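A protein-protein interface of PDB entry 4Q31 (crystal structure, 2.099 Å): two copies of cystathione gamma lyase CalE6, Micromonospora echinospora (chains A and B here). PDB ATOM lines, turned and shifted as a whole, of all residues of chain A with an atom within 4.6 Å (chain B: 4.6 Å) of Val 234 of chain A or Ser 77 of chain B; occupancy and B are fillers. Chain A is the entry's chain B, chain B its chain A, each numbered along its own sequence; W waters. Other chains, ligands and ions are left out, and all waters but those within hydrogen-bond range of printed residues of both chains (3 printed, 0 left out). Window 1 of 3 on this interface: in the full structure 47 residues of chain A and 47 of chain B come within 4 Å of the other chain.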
ATOM      1  N   ARG A  51      -5.702  16.807 -24.406  1.00  0.00           N
ATOM      2  CA  ARG A  51      -5.084  15.651 -25.058  1.00  0.00           C
ATOM      3  C   ARG A  51      -3.605  15.578 -24.675  1.00  0.00           C
ATOM      4  O   ARG A  51      -3.049  14.490 -24.504  1.00  0.00           O
ATOM      5  CB  ARG A  51      -5.256  15.686 -26.588  1.00  0.00           C
ATOM      6  CG  ARG A  51      -4.480  14.571 -27.331  1.00  0.00           C
ATOM      7  CD  ARG A  51      -5.019  14.282 -28.738  1.00  0.00           C
ATOM      8  NE  ARG A  51      -5.618  15.456 -29.376  1.00  0.00           N
ATOM      9  CZ  ARG A  51      -4.931  16.439 -29.947  1.00  0.00           C
ATOM     10  NH1 ARG A  51      -5.575  17.469 -30.489  1.00  0.00           N
ATOM     11  NH2 ARG A  51      -3.601  16.405 -29.956  1.00  0.00           N
ATOM     12  N   ARG A  57      -4.587  12.606 -14.987  1.00  0.00           N
ATOM     13  CA  ARG A  57      -3.856  11.562 -15.703  1.00  0.00           C
ATOM     14  C   ARG A  57      -2.383  11.487 -15.248  1.00  0.00           C
ATOM     15  O   ARG A  57      -1.830  10.401 -15.076  1.00  0.00           O
ATOM     16  CB  ARG A  57      -3.971  11.802 -17.214  1.00  0.00           C
ATOM     17  CG  ARG A  57      -3.198  10.848 -18.088  1.00  0.00           C
ATOM     18  CD  ARG A  57      -3.570  11.056 -19.549  1.00  0.00           C
ATOM     19  NE  ARG A  57      -2.929  12.250 -20.090  1.00  0.00           N
ATOM     20  CZ  ARG A  57      -3.576  13.220 -20.729  1.00  0.00           C
ATOM     21  NH1 ARG A  57      -4.890  13.141 -20.918  1.00  0.00           N
ATOM     22  NH2 ARG A  57      -2.903  14.264 -21.182  1.00  0.00           N
ATOM     23  N   SER A  77      -5.737   4.847 -23.488  1.00  0.00           N
ATOM     24  CA  SER A  77      -7.142   4.475 -23.502  1.00  0.00           C
ATOM     25  C   SER A  77      -7.396   2.968 -23.331  1.00  0.00           C
ATOM     26  O   SER A  77      -8.509   2.560 -22.996  1.00  0.00           O
ATOM     27  CB  SER A  77      -7.776   4.979 -24.808  1.00  0.00           C
ATOM     28  OG  SER A  77      -7.007   4.560 -25.921  1.00  0.00           O
ATOM     29  N   ARG A 228       1.372   9.453 -28.475  1.00  0.00           N
ATOM     30  CA  ARG A 228       0.081   9.485 -27.810  1.00  0.00           C
ATOM     31  C   ARG A 228      -0.664  10.759 -28.187  1.00  0.00           C
ATOM     32  O   ARG A 228      -1.856  10.733 -28.484  1.00  0.00           O
ATOM     33  CB  ARG A 228       0.232   9.401 -26.286  1.00  0.00           C
ATOM     34  CG  ARG A 228      -1.125   9.183 -25.591  1.00  0.00           C
ATOM     35  CD  ARG A 228      -1.029   9.188 -24.067  1.00  0.00           C
ATOM     36  NE  ARG A 228      -0.540  10.467 -23.586  1.00  0.00           N
ATOM     37  CZ  ARG A 228      -0.351  10.757 -22.306  1.00  0.00           C
ATOM     38  NH1 ARG A 228      -0.633   9.854 -21.366  1.00  0.00           N
ATOM     39  NH2 ARG A 228       0.102  11.958 -21.967  1.00  0.00           N
ATOM     40  N   GLY A 232      -3.703  10.247 -30.409  1.00  0.00           N
ATOM     41  CA  GLY A 232      -4.848  10.640 -29.595  1.00  0.00           C
ATOM     42  C   GLY A 232      -5.484   9.502 -28.822  1.00  0.00           C
ATOM     43  O   GLY A 232      -6.666   9.569 -28.462  1.00  0.00           O
ATOM     44  N   ASN A 233      -4.703   8.452 -28.573  1.00  0.00           N
ATOM     45  CA  ASN A 233      -5.183   7.304 -27.814  1.00  0.00           C
ATOM     46  C   ASN A 233      -5.065   7.548 -26.309  1.00  0.00           C
ATOM     47  O   ASN A 233      -4.533   6.718 -25.563  1.00  0.00           O
ATOM     48  CB  ASN A 233      -4.454   6.013 -28.234  1.00  0.00           C
ATOM     49  CG  ASN A 233      -2.930   6.167 -28.272  1.00  0.00           C
ATOM     50  OD1 ASN A 233      -2.373   7.207 -27.900  1.00  0.00           O
ATOM     51  ND2 ASN A 233      -2.250   5.115 -28.721  1.00  0.00           N
ATOM     52  N   VAL A 234      -5.574   8.696 -25.874  1.00  0.00           N
ATOM     53  CA  VAL A 234      -5.475   9.127 -24.478  1.00  0.00           C
ATOM     54  C   VAL A 234      -6.716   8.725 -23.702  1.00  0.00           C
ATOM     55  O   VAL A 234      -7.806   8.755 -24.253  1.00  0.00           O
ATOM     56  CB  VAL A 234      -5.364  10.652 -24.397  1.00  0.00           C
ATOM     57  CG1 VAL A 234      -4.027  11.100 -24.882  1.00  0.00           C
ATOM     58  CG2 VAL A 234      -6.448  11.298 -25.246  1.00  0.00           C
ATOM     59  N   PRO A 235      -6.553   8.330 -22.422  1.00  0.00           N
ATOM     60  CA  PRO A 235      -7.719   7.974 -21.596  1.00  0.00           C
ATOM     61  C   PRO A 235      -8.375   9.242 -21.048  1.00  0.00           C
ATOM     62  O   PRO A 235      -7.737  10.293 -20.999  1.00  0.00           O
ATOM     63  CB  PRO A 235      -7.093   7.165 -20.437  1.00  0.00           C
ATOM     64  CG  PRO A 235      -5.771   7.825 -20.217  1.00  0.00           C
ATOM     65  CD  PRO A 235      -5.299   8.304 -21.644  1.00  0.00           C
ATOM     66  N   GLY A 236      -9.633   9.156 -20.642  1.00  0.00           N
ATOM     67  CA  GLY A 236     -10.303  10.307 -20.066  1.00  0.00           C
ATOM     68  C   GLY A 236      -9.960  10.480 -18.595  1.00  0.00           C
ATOM     69  O   GLY A 236      -9.417   9.568 -17.965  1.00  0.00           O
ATOM     70  N   PHE B  76     -14.444   7.606 -30.881  1.00  0.00           N
ATOM     71  CA  PHE B  76     -13.045   7.396 -30.547  1.00  0.00           C
ATOM     72  C   PHE B  76     -12.642   8.193 -29.316  1.00  0.00           C
ATOM     73  O   PHE B  76     -13.375   9.094 -28.887  1.00  0.00           O
ATOM     74  CB  PHE B  76     -12.197   7.820 -31.748  1.00  0.00           C
ATOM     75  CG  PHE B  76     -12.423   6.962 -32.971  1.00  0.00           C
ATOM     76  CD1 PHE B  76     -13.427   7.275 -33.883  1.00  0.00           C
ATOM     77  CD2 PHE B  76     -11.649   5.826 -33.189  1.00  0.00           C
ATOM     78  CE1 PHE B  76     -13.638   6.472 -35.013  1.00  0.00           C
ATOM     79  CE2 PHE B  76     -11.849   5.018 -34.312  1.00  0.00           C
ATOM     80  CZ  PHE B  76     -12.842   5.343 -35.222  1.00  0.00           C
ATOM     81  N   SER B  77     -11.478   7.864 -28.752  1.00  0.00           N
ATOM     82  CA  SER B  77     -10.952   8.573 -27.580  1.00  0.00           C
ATOM     83  C   SER B  77     -10.662  10.063 -27.818  1.00  0.00           C
ATOM     84  O   SER B  77     -10.507  10.831 -26.862  1.00  0.00           O
ATOM     85  CB  SER B  77      -9.693   7.869 -27.052  1.00  0.00           C
ATOM     86  OG  SER B  77      -8.772   7.631 -28.107  1.00  0.00           O
ATOM     87  N   SER B  78     -10.578  10.469 -29.083  1.00  0.00           N
ATOM     88  CA  SER B  78     -10.282  11.864 -29.417  1.00  0.00           C
ATOM     89  C   SER B  78     -10.518  12.075 -30.893  1.00  0.00           C
ATOM     90  O   SER B  78     -10.610  11.108 -31.639  1.00  0.00           O
ATOM     91  CB  SER B  78      -8.827  12.226 -29.092  1.00  0.00           C
ATOM     92  OG  SER B  78      -7.916  11.506 -29.912  1.00  0.00           O
ATOM     93  N   ALA B  81      -7.747  10.534 -32.872  1.00  0.00           N
ATOM     94  CA  ALA B  81      -7.865   9.085 -33.013  1.00  0.00           C
ATOM     95  C   ALA B  81      -8.797   8.697 -34.151  1.00  0.00           C
ATOM     96  O   ALA B  81      -8.563   7.709 -34.841  1.00  0.00           O
ATOM     97  CB  ALA B  81      -8.322   8.447 -31.702  1.00  0.00           C
ATOM     98  N   LEU B 209     -12.823  14.601 -23.840  1.00  0.00           N
ATOM     99  CA  LEU B 209     -12.200  14.432 -25.166  1.00  0.00           C
ATOM    100  C   LEU B 209     -12.910  13.344 -25.937  1.00  0.00           C
ATOM    101  O   LEU B 209     -13.321  12.336 -25.357  1.00  0.00           O
ATOM    102  CB  LEU B 209     -10.738  14.027 -25.030  1.00  0.00           C
ATOM    103  CG  LEU B 209      -9.786  15.001 -24.349  1.00  0.00           C
ATOM    104  CD1 LEU B 209      -8.516  14.270 -23.924  1.00  0.00           C
ATOM    105  CD2 LEU B 209      -9.462  16.140 -25.308  1.00  0.00           C
ATOM    106  N   GLY B 210     -13.040  13.513 -27.249  1.00  0.00           N
ATOM    107  CA  GLY B 210     -13.662  12.467 -28.050  1.00  0.00           C
ATOM    108  C   GLY B 210     -13.572  12.745 -29.534  1.00  0.00           C
ATOM    109  O   GLY B 210     -13.360  13.888 -29.939  1.00  0.00           O
ATOM    110  N   GLY B 211     -13.723  11.703 -30.347  1.00  0.00           N
ATOM    111  CA  GLY B 211     -13.745  11.875 -31.793  1.00  0.00           C
ATOM    112  C   GLY B 211     -14.851  11.022 -32.380  1.00  0.00           C
ATOM    113  O   GLY B 211     -15.428  10.185 -31.683  1.00  0.00           O
ATOM    114  N   ASN B 233      -8.079   2.556 -29.496  1.00  0.00           N
ATOM    115  CA  ASN B 233      -8.306   3.982 -29.306  1.00  0.00           C
ATOM    116  C   ASN B 233      -9.779   4.234 -29.055  1.00  0.00           C
ATOM    117  O   ASN B 233     -10.410   5.044 -29.734  1.00  0.00           O
ATOM    118  CB  ASN B 233      -7.764   4.807 -30.497  1.00  0.00           C
ATOM    119  CG  ASN B 233      -8.266   4.302 -31.859  1.00  0.00           C
ATOM    120  OD1 ASN B 233      -9.102   3.396 -31.928  1.00  0.00           O
ATOM    121  ND2 ASN B 233      -7.754   4.899 -32.949  1.00  0.00           N
ATOM    122  N   VAL B 234     -10.321   3.525 -28.061  1.00  0.00           N
ATOM    123  CA  VAL B 234     -11.740   3.590 -27.726  1.00  0.00           C
ATOM    124  C   VAL B 234     -11.988   4.553 -26.578  1.00  0.00           C
ATOM    125  O   VAL B 234     -11.186   4.623 -25.656  1.00  0.00           O
ATOM    126  CB  VAL B 234     -12.266   2.207 -27.271  1.00  0.00           C
ATOM    127  CG1 VAL B 234     -12.387   1.267 -28.446  1.00  0.00           C
ATOM    128  CG2 VAL B 234     -11.345   1.610 -26.222  1.00  0.00           C
ATOM    129  N   PRO B 235     -13.116   5.286 -26.613  1.00  0.00           N
ATOM    130  CA  PRO B 235     -13.493   6.162 -25.491  1.00  0.00           C
ATOM    131  C   PRO B 235     -14.114   5.396 -24.314  1.00  0.00           C
ATOM    132  O   PRO B 235     -14.687   4.316 -24.496  1.00  0.00           O
ATOM    133  CB  PRO B 235     -14.564   7.060 -26.113  1.00  0.00           C
ATOM    134  CG  PRO B 235     -15.246   6.167 -27.111  1.00  0.00           C
ATOM    135  CD  PRO B 235     -14.173   5.215 -27.639  1.00  0.00           C
HETATM  136  O   HOH W   1     -10.365  10.446 -24.204  1.00  0.00           O
HETATM  137  O   HOH W   2     -10.997   3.760 -22.775  1.00  0.00           O
HETATM  138  O   HOH W   3     -10.300   6.736 -23.830  1.00  0.00           O
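Leu 209 of chain B touches Arg 51 of chain A (CD1 to N, 3.8 Å). CA of Asn 233 of chain B touches OG of Ser 77 of chain A, 3.7 Å away. Val 234 of chain B touches Ser 77 of chain A (O to CB, 3.5 Å). Gly 232 of chain A touches Ala 81 of chain B. Ser 77 of chain B touches Asn 233 of chain A (OG to CA, 3.6 Å). CB of Ser 77 of chain B touches O of Val 234 of chain A, at 3.5 Å. Val 234 of chain A touches Leu 209 of chain B.
Water W1 lies within hydrogen-bond range of O of Ser 77 of chain B and O of Val 234 of chain A. Water W2 bridges O of Ser 77 of chain A (2.8 Å) and O of Val 234 of chain B (3.0 Å). Water W3 bridges O of Val 234 of chain B and O of Val 234 of chain A.
Of the 9 printed residues of chain A, 5 touch a printed residue of chain B. Printed residues of chain A that touch a printed residue of chain B: Arg 51, Ser 77, Gly 232, Asn 233 and Val 234. Among the printed residues, 9 pairs touch across the chains.
Ser 77 of chain A touches Asn 233 of chain B, and with the chains exchanged Asn 233 of chain A touches Ser 77 of chain B. Ser 77 of chain A touches Val 234 of chain B, and with the chains exchanged Val 234 of chain A touches Ser 77 of chain B. Of the 9 pairs that touch across the chains among the printed residues, 4 have their exchanged pair printed and touching as well.
OG of Ser 78 of chain B is in hydrogen-bond range of O of Gly 232 of chain A (2.7 Å). O of Gly 232 of chain A sits at hydrogen-bond distance from OG of Ser 77 of chain B (2.9 Å).
Printed residues of chain B within 4 Å of Ser 77 of chain A: Asn 233 (3.7 Å) and Val 234 (3.5 Å). Printed residues of chain B within 4 Å of Gly 232 of chain A: Ser 77 (2.9 Å), Ser 78 (2.7 Å) and Ala 81 (3.8 Å). Printed residues of chain B within 4 Å of Asn 233 of chain A: Ser 77. Val 234 of chain A touches just these residues of chain B: Ser 77 and Leu 209. Pro 235 of chain A touches none of the printed residues of chain B. Of the printed residues of chain A, Ser 78 of chain B touches Gly 232. Of the printed residues of chain A, Ala 81 of chain B touches Gly 232 (3.8 Å). The nearest residue of chain A that does not touch Ser 77 of chain B is Ser 77 of chain A (4.1 Å).
N of Ser 77 of chain A is in hydrogen-bond range of O of Asn 233 of chain A (3.0 Å). N of Ser 77 of chain B is in hydrogen-bond range of O of Asn 233 of chain B (3.2 Å). The backbone NH of Ala 81 of chain B sits at hydrogen-bond distance from the side-chain hydroxyl of Ser 78 of chain B (3.1 Å). The backbone carbonyl oxygen (O) of Ala 81 of chain B is in hydrogen-bond range of the side-chain amide nitrogen (ND2) of Asn 233 of chain B, at 3.5 Å. The backbone carbonyl oxygen of Arg 51 of chain A is in hydrogen-bond range of the guanidinium group of Arg 57 of chain A (3.3 Å). N of Gly 211 of chain B lies close to O of Ser 78 of chain B, at 3.4 Å.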
